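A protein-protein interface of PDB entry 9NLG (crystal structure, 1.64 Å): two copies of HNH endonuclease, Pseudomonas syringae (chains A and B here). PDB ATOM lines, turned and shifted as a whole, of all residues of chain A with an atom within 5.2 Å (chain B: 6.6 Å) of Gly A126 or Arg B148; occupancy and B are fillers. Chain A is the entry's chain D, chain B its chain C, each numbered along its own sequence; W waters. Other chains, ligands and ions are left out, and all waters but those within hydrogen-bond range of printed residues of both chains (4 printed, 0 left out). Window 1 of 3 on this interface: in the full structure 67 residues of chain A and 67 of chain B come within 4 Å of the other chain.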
ATOM      1  N   LEU A 119     -30.627 -25.145 -18.112  1.00  0.00           N
ATOM      2  CA  LEU A 119     -30.523 -25.899 -16.866  1.00  0.00           C
ATOM      3  C   LEU A 119     -31.228 -27.236 -16.994  1.00  0.00           C
ATOM      4  O   LEU A 119     -30.724 -28.262 -16.531  1.00  0.00           O
ATOM      5  CB  LEU A 119     -31.106 -25.080 -15.729  1.00  0.00           C
ATOM      6  CG  LEU A 119     -30.961 -25.667 -14.334  1.00  0.00           C
ATOM      7  CD1 LEU A 119     -29.505 -25.783 -13.942  1.00  0.00           C
ATOM      8  CD2 LEU A 119     -31.731 -24.783 -13.362  1.00  0.00           C
ATOM      9  N   THR A 122     -29.127 -29.657 -19.420  1.00  0.00           N
ATOM     10  CA  THR A 122     -27.899 -30.215 -18.866  1.00  0.00           C
ATOM     11  C   THR A 122     -28.146 -31.120 -17.662  1.00  0.00           C
ATOM     12  O   THR A 122     -27.194 -31.674 -17.103  1.00  0.00           O
ATOM     13  CB  THR A 122     -26.921 -29.108 -18.453  1.00  0.00           C
ATOM     14  OG1 THR A 122     -27.508 -28.287 -17.437  1.00  0.00           O
ATOM     15  CG2 THR A 122     -26.520 -28.243 -19.650  1.00  0.00           C
ATOM     16  N   THR A 123     -29.414 -31.288 -17.254  1.00  0.00           N
ATOM     17  CA  THR A 123     -29.682 -32.077 -16.060  1.00  0.00           C
ATOM     18  C   THR A 123     -29.105 -33.482 -16.117  1.00  0.00           C
ATOM     19  O   THR A 123     -28.756 -33.999 -15.033  1.00  0.00           O
ATOM     20  CB  THR A 123     -31.209 -32.119 -15.848  1.00  0.00           C
ATOM     21  OG1 THR A 123     -31.697 -30.789 -15.654  1.00  0.00           O
ATOM     22  CG2 THR A 123     -31.566 -32.957 -14.628  1.00  0.00           C
ATOM     23  N   PRO A 124     -28.957 -34.141 -17.260  1.00  0.00           N
ATOM     24  CA  PRO A 124     -28.338 -35.468 -17.242  1.00  0.00           C
ATOM     25  C   PRO A 124     -26.954 -35.476 -16.619  1.00  0.00           C
ATOM     26  O   PRO A 124     -26.534 -36.528 -16.109  1.00  0.00           O
ATOM     27  CB  PRO A 124     -28.300 -35.859 -18.725  1.00  0.00           C
ATOM     28  CG  PRO A 124     -29.465 -35.141 -19.306  1.00  0.00           C
ATOM     29  CD  PRO A 124     -29.501 -33.810 -18.596  1.00  0.00           C
ATOM     30  N   ASP A 125     -26.226 -34.359 -16.617  1.00  0.00           N
ATOM     31  CA  ASP A 125     -24.903 -34.383 -15.997  1.00  0.00           C
ATOM     32  C   ASP A 125     -24.970 -34.270 -14.482  1.00  0.00           C
ATOM     33  O   ASP A 125     -23.949 -34.481 -13.818  1.00  0.00           O
ATOM     34  CB  ASP A 125     -23.994 -33.319 -16.658  1.00  0.00           C
ATOM     35  CG  ASP A 125     -23.964 -31.960 -15.947  1.00  0.00           C
ATOM     36  OD1 ASP A 125     -24.327 -31.805 -14.762  1.00  0.00           O
ATOM     37  OD2 ASP A 125     -23.516 -31.009 -16.623  1.00  0.00           O
ATOM     38  N   GLY A 126     -26.144 -33.995 -13.917  1.00  0.00           N
ATOM     39  CA  GLY A 126     -26.375 -34.151 -12.493  1.00  0.00           C
ATOM     40  C   GLY A 126     -26.432 -35.585 -12.026  1.00  0.00           C
ATOM     41  O   GLY A 126     -26.573 -35.832 -10.824  1.00  0.00           O
ATOM     42  N   GLY A 127     -26.324 -36.534 -12.949  1.00  0.00           N
ATOM     43  CA  GLY A 127     -26.340 -37.939 -12.644  1.00  0.00           C
ATOM     44  C   GLY A 127     -24.985 -38.560 -12.396  1.00  0.00           C
ATOM     45  O   GLY A 127     -24.936 -39.761 -12.112  1.00  0.00           O
ATOM     46  N   ARG A 128     -23.883 -37.802 -12.489  1.00  0.00           N
ATOM     47  CA  ARG A 128     -22.566 -38.357 -12.180  1.00  0.00           C
ATOM     48  C   ARG A 128     -22.609 -39.060 -10.829  1.00  0.00           C
ATOM     49  O   ARG A 128     -23.078 -38.489  -9.843  1.00  0.00           O
ATOM     50  CB  ARG A 128     -21.506 -37.255 -12.156  1.00  0.00           C
ATOM     51  CG  ARG A 128     -21.082 -36.762 -13.522  1.00  0.00           C
ATOM     52  CD  ARG A 128     -19.862 -35.807 -13.445  1.00  0.00           C
ATOM     53  NE  ARG A 128     -18.549 -36.443 -13.318  1.00  0.00           N
ATOM     54  CZ  ARG A 128     -17.788 -36.406 -12.226  1.00  0.00           C
ATOM     55  NH1 ARG A 128     -18.237 -35.899 -11.094  1.00  0.00           N
ATOM     56  NH2 ARG A 128     -16.544 -36.873 -12.286  1.00  0.00           N
ATOM     57  N   THR A 204     -21.586 -29.613 -14.655  1.00  0.00           N
ATOM     58  CA  THR A 204     -21.627 -28.203 -15.044  1.00  0.00           C
ATOM     59  C   THR A 204     -21.163 -27.281 -13.921  1.00  0.00           C
ATOM     60  O   THR A 204     -20.603 -26.213 -14.195  1.00  0.00           O
ATOM     61  CB  THR A 204     -23.046 -27.832 -15.490  1.00  0.00           C
ATOM     62  OG1 THR A 204     -23.383 -28.595 -16.662  1.00  0.00           O
ATOM     63  CG2 THR A 204     -23.181 -26.339 -15.788  1.00  0.00           C
ATOM     64  N   TYR A 205     -21.360 -27.676 -12.662  1.00  0.00           N
ATOM     65  CA  TYR A 205     -21.179 -26.778 -11.527  1.00  0.00           C
ATOM     66  C   TYR A 205     -20.102 -27.221 -10.551  1.00  0.00           C
ATOM     67  O   TYR A 205     -19.927 -26.577  -9.513  1.00  0.00           O
ATOM     68  CB  TYR A 205     -22.515 -26.623 -10.786  1.00  0.00           C
ATOM     69  CG  TYR A 205     -23.604 -26.096 -11.687  1.00  0.00           C
ATOM     70  CD1 TYR A 205     -23.588 -24.774 -12.119  1.00  0.00           C
ATOM     71  CD2 TYR A 205     -24.629 -26.917 -12.130  1.00  0.00           C
ATOM     72  CE1 TYR A 205     -24.572 -24.281 -12.956  1.00  0.00           C
ATOM     73  CE2 TYR A 205     -25.620 -26.431 -12.963  1.00  0.00           C
ATOM     74  CZ  TYR A 205     -25.579 -25.115 -13.382  1.00  0.00           C
ATOM     75  OH  TYR A 205     -26.561 -24.626 -14.207  1.00  0.00           O
ATOM     76  N   ASP A 207     -20.123 -30.029  -8.815  1.00  0.00           N
ATOM     77  CA  ASP A 207     -20.677 -30.796  -7.712  1.00  0.00           C
ATOM     78  C   ASP A 207     -19.946 -32.126  -7.541  1.00  0.00           C
ATOM     79  O   ASP A 207     -19.486 -32.737  -8.510  1.00  0.00           O
ATOM     80  CB  ASP A 207     -22.166 -31.069  -7.946  1.00  0.00           C
ATOM     81  CG  ASP A 207     -23.056 -29.858  -7.685  1.00  0.00           C
ATOM     82  OD1 ASP A 207     -22.719 -29.032  -6.808  1.00  0.00           O
ATOM     83  OD2 ASP A 207     -24.108 -29.752  -8.351  1.00  0.00           O
ATOM     84  N   LYS A 234     -26.225 -36.014  -1.863  1.00  0.00           N
ATOM     85  CA  LYS A 234     -26.950 -36.688  -2.933  1.00  0.00           C
ATOM     86  C   LYS A 234     -26.564 -38.166  -2.934  1.00  0.00           C
ATOM     87  O   LYS A 234     -25.441 -38.534  -3.297  1.00  0.00           O
ATOM     88  CB  LYS A 234     -26.686 -36.055  -4.292  1.00  0.00           C
ATOM     89  CG  LYS A 234     -27.588 -36.672  -5.370  1.00  0.00           C
ATOM     90  CD  LYS A 234     -27.638 -35.880  -6.668  1.00  0.00           C
ATOM     91  CE  LYS A 234     -28.377 -36.668  -7.751  1.00  0.00           C
ATOM     92  NZ  LYS A 234     -28.860 -35.817  -8.880  1.00  0.00           N
ATOM     93  N   CYS B  35     -26.200 -37.518 -21.606  1.00  0.00           N
ATOM     94  CA  CYS B  35     -25.143 -36.882 -20.825  1.00  0.00           C
ATOM     95  C   CYS B  35     -25.264 -35.370 -20.693  1.00  0.00           C
ATOM     96  O   CYS B  35     -24.481 -34.771 -19.943  1.00  0.00           O
ATOM     97  CB  CYS B  35     -23.757 -37.210 -21.406  1.00  0.00           C
ATOM     98  SG  CYS B  35     -23.319 -36.359 -22.930  1.00  0.00           S
ATOM     99  N   ILE B 133     -25.905 -21.264  -0.726  1.00  0.00           N
ATOM    100  CA  ILE B 133     -25.828 -22.512   0.024  1.00  0.00           C
ATOM    101  C   ILE B 133     -24.908 -22.280   1.217  1.00  0.00           C
ATOM    102  O   ILE B 133     -23.786 -21.796   1.052  1.00  0.00           O
ATOM    103  CB  ILE B 133     -25.299 -23.660  -0.855  1.00  0.00           C
ATOM    104  CG1 ILE B 133     -26.293 -23.966  -1.974  1.00  0.00           C
ATOM    105  CG2 ILE B 133     -25.006 -24.895  -0.007  1.00  0.00           C
ATOM    106  CD1 ILE B 133     -25.779 -24.952  -3.003  1.00  0.00           C
ATOM    107  N   ILE B 145     -24.641 -30.038  -0.105  1.00  0.00           N
ATOM    108  CA  ILE B 145     -25.815 -29.669  -0.888  1.00  0.00           C
ATOM    109  C   ILE B 145     -25.372 -29.406  -2.327  1.00  0.00           C
ATOM    110  O   ILE B 145     -24.569 -28.489  -2.555  1.00  0.00           O
ATOM    111  CB  ILE B 145     -26.511 -28.434  -0.302  1.00  0.00           C
ATOM    112  CG1 ILE B 145     -26.966 -28.699   1.139  1.00  0.00           C
ATOM    113  CG2 ILE B 145     -27.681 -28.031  -1.194  1.00  0.00           C
ATOM    114  CD1 ILE B 145     -27.538 -27.484   1.848  1.00  0.00           C
ATOM    115  N   PRO B 146     -25.878 -30.151  -3.313  1.00  0.00           N
ATOM    116  CA  PRO B 146     -25.466 -29.898  -4.701  1.00  0.00           C
ATOM    117  C   PRO B 146     -25.954 -28.547  -5.204  1.00  0.00           C
ATOM    118  O   PRO B 146     -27.111 -28.161  -5.002  1.00  0.00           O
ATOM    119  CB  PRO B 146     -26.117 -31.049  -5.491  1.00  0.00           C
ATOM    120  CG  PRO B 146     -26.484 -32.077  -4.452  1.00  0.00           C
ATOM    121  CD  PRO B 146     -26.767 -31.324  -3.205  1.00  0.00           C
ATOM    122  N   VAL B 147     -25.045 -27.825  -5.873  1.00  0.00           N
ATOM    123  CA  VAL B 147     -25.406 -26.554  -6.493  1.00  0.00           C
ATOM    124  C   VAL B 147     -26.525 -26.752  -7.508  1.00  0.00           C
ATOM    125  O   VAL B 147     -27.475 -25.964  -7.565  1.00  0.00           O
ATOM    126  CB  VAL B 147     -24.161 -25.915  -7.135  1.00  0.00           C
ATOM    127  CG1 VAL B 147     -24.543 -24.675  -7.940  1.00  0.00           C
ATOM    128  CG2 VAL B 147     -23.124 -25.573  -6.075  1.00  0.00           C
ATOM    129  N   ARG B 148     -26.428 -27.798  -8.338  1.00  0.00           N
ATOM    130  CA  ARG B 148     -27.436 -27.995  -9.375  1.00  0.00           C
ATOM    131  C   ARG B 148     -28.827 -28.085  -8.762  1.00  0.00           C
ATOM    132  O   ARG B 148     -29.797 -27.567  -9.317  1.00  0.00           O
ATOM    133  CB  ARG B 148     -27.138 -29.241 -10.210  1.00  0.00           C
ATOM    134  CG  ARG B 148     -28.243 -29.584 -11.215  1.00  0.00           C
ATOM    135  CD  ARG B 148     -27.856 -30.682 -12.206  1.00  0.00           C
ATOM    136  NE  ARG B 148     -26.871 -30.249 -13.187  1.00  0.00           N
ATOM    137  CZ  ARG B 148     -27.148 -29.573 -14.295  1.00  0.00           C
ATOM    138  NH1 ARG B 148     -28.388 -29.210 -14.596  1.00  0.00           N
ATOM    139  NH2 ARG B 148     -26.155 -29.268 -15.129  1.00  0.00           N
ATOM    140  N   ASP B 149     -28.941 -28.704  -7.587  1.00  0.00           N
ATOM    141  CA  ASP B 149     -30.272 -28.920  -7.029  1.00  0.00           C
ATOM    142  C   ASP B 149     -30.899 -27.626  -6.526  1.00  0.00           C
ATOM    143  O   ASP B 149     -32.113 -27.446  -6.660  1.00  0.00           O
ATOM    144  CB  ASP B 149     -30.208 -29.993  -5.951  1.00  0.00           C
ATOM    145  CG  ASP B 149     -30.031 -31.372  -6.557  1.00  0.00           C
ATOM    146  OD1 ASP B 149     -28.877 -31.764  -6.819  1.00  0.00           O
ATOM    147  OD2 ASP B 149     -31.059 -32.024  -6.865  1.00  0.00           O
ATOM    148  N   LEU B 150     -30.104 -26.711  -5.965  1.00  0.00           N
ATOM    149  CA  LEU B 150     -30.660 -25.403  -5.628  1.00  0.00           C
ATOM    150  C   LEU B 150     -31.098 -24.660  -6.886  1.00  0.00           C
ATOM    151  O   LEU B 150     -32.208 -24.118  -6.948  1.00  0.00           O
ATOM    152  CB  LEU B 150     -29.665 -24.557  -4.835  1.00  0.00           C
ATOM    153  CG  LEU B 150     -30.157 -23.141  -4.513  1.00  0.00           C
ATOM    154  CD1 LEU B 150     -31.459 -23.149  -3.729  1.00  0.00           C
ATOM    155  CD2 LEU B 150     -29.077 -22.357  -3.747  1.00  0.00           C
ATOM    156  N   LEU B 151     -30.239 -24.630  -7.908  1.00  0.00           N
ATOM    157  CA  LEU B 151     -30.591 -23.930  -9.144  1.00  0.00           C
ATOM    158  C   LEU B 151     -31.850 -24.513  -9.773  1.00  0.00           C
ATOM    159  O   LEU B 151     -32.675 -23.773 -10.320  1.00  0.00           O
ATOM    160  CB  LEU B 151     -29.425 -23.977 -10.126  1.00  0.00           C
ATOM    161  CG  LEU B 151     -28.152 -23.262  -9.670  1.00  0.00           C
ATOM    162  CD1 LEU B 151     -27.013 -23.563 -10.634  1.00  0.00           C
ATOM    163  CD2 LEU B 151     -28.344 -21.762  -9.536  1.00  0.00           C
ATOM    164  N   THR B 152     -32.028 -25.832  -9.685  1.00  0.00           N
ATOM    165  CA  THR B 152     -33.207 -26.458 -10.276  1.00  0.00           C
ATOM    166  C   THR B 152     -34.469 -26.135  -9.485  1.00  0.00           C
ATOM    167  O   THR B 152     -35.528 -25.887 -10.079  1.00  0.00           O
ATOM    168  CB  THR B 152     -32.988 -27.964 -10.400  1.00  0.00           C
ATOM    169  OG1 THR B 152     -32.663 -28.522  -9.127  1.00  0.00           O
ATOM    170  CG2 THR B 152     -31.860 -28.219 -11.354  1.00  0.00           C
ATOM    171  N   ALA B 153     -34.371 -26.097  -8.152  1.00  0.00           N
ATOM    172  CA  ALA B 153     -35.508 -25.664  -7.340  1.00  0.00           C
ATOM    173  C   ALA B 153     -35.834 -24.201  -7.606  1.00  0.00           C
ATOM    174  O   ALA B 153     -37.009 -23.816  -7.664  1.00  0.00           O
ATOM    175  CB  ALA B 153     -35.218 -25.891  -5.857  1.00  0.00           C
HETATM  176  O   HOH W   1     -31.022 -34.462  -7.935  1.00  0.00           O
HETATM  177  O   HOH W   2     -24.489 -31.232 -11.894  1.00  0.00           O
HETATM  178  O   HOH W   3     -30.914 -29.980 -13.315  1.00  0.00           O
HETATM  179  O   HOH W   4     -27.728 -32.895  -8.991  1.00  0.00           O
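The backbone NH (N) of Val B147 lies within hydrogen-bond range of the side-chain carboxylate (OD1) of Asp A207, at 2.8 Å.
The backbone carbonyl oxygen (O) of Leu A119 sits at hydrogen-bond distance from the guanidinium group (NH1) of Arg B148 (3.2 Å).
The guanidinium group of Arg B148 lies within hydrogen-bond range of the side-chain hydroxyl of Thr A122, at 2.8 Å.
The side-chain carboxylate (OD1) of Asp A125 is in salt-bridge range of the guanidinium group (NH2) of Arg B148 (3.1 Å).
The guanidinium group of Arg B148 lies within hydrogen-bond range of the side-chain hydroxyl of Thr A204.
N of Arg B148 is in hydrogen-bond range of OD2 of Asp A207 (3.0 Å).
O of Arg B148 sits close to OG1 of Thr B152, at 3.0 Å.
The side-chain hydroxyl (OG1) of Thr B152 sits at hydrogen-bond distance from the backbone carbonyl oxygen (O) of Asp B149, 2.7 Å away.
The backbone carbonyl oxygen (O) of Leu A119 is in hydrogen-bond range of the side-chain hydroxyl (OG1) of Thr A122 (3.3 Å).
The side-chain hydroxyl (OG1) of Thr A123 lies within hydrogen-bond range of the backbone carbonyl oxygen (O) of Leu A119 (2.8 Å).
OD2 of Asp A125 is in hydrogen-bond range of OG1 of Thr A204 (2.4 Å).
The side-chain amino group (NZ) of Lys A234 lies within hydrogen-bond range of the backbone carbonyl oxygen (O) of Gly A126, at 3.0 Å.
Among the printed residues, pairs that only touch across the chains: Leu A119 with Leu B151, Tyr A205 with Leu B151, Thr A123 with Arg B148, Asp A207 with Pro B146, Tyr A205 with Arg B148, Asp A125 with Cys B35, Pro A124 with Cys B35, Gly A126 with Arg B148, Leu A119 with Thr B152 and Lys A234 with Pro B146.
Of chain A, only Leu A119 (3.2 Å), Thr A122 (2.8 Å), Thr A123 (3.5 Å), Asp A125 (3.1 Å), Gly A126 (3.8 Å), Thr A204 (3.2 Å), Tyr A205 (3.6 Å) and Asp A207 (3.0 Å) come within 4 Å of Arg B148.
Of the printed residues of chain A, Val B147 touches Asp A207.
Of the printed residues of chain B, Thr A204 touches Arg B148.
Of the printed residues of chain B, Thr A122 touches Arg B148 (2.8 Å).
Of the printed residues of chain B, Tyr A205 touches Arg B148 and Leu B151.
The nearest printed residue of chain B that does not touch Pro A124 is Arg B148 (5.6 Å).
Of the 12 printed residues of chain A, 10 touch a printed residue of chain B.
Printed residues of chain B that touch a printed residue of chain A: Cys B35, Pro B146, Val B147, Arg B148, Leu B151 and Thr B152.
Hydrophobic or aromatic side chains of chain B that line the printed part of chain A: Pro B146, Val B147 and Leu B151.
Among the printed residues, Asp or Glu carboxylates within 4 Å of a Lys or Arg side-chain nitrogen of the other chain: Asp A125 with Arg B148.
No position is printed for both chains.
Of the 16 pairs that touch across the chains among the printed residues, none has its exchanged pair printed and touching as well.
Water W3 bridges the side-chain hydroxyl (OG1) of Thr A123 (2.6 Å) and the guanidinium group (NH1) of Arg B148 (2.9 Å).
Water W1 lies within hydrogen-bond range of OD2 of Asp B149 and NZ of Lys A234.
Water W4 lies within hydrogen-bond range of OD1 of Asp B149 (2.7 Å) and NZ of Lys A234 (3.1 Å).
Water W2 bridges the guanidinium group (NE) of Arg B148 (2.9 Å) and the side-chain carboxylate (OD1) of Asp A125 (2.9 Å).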
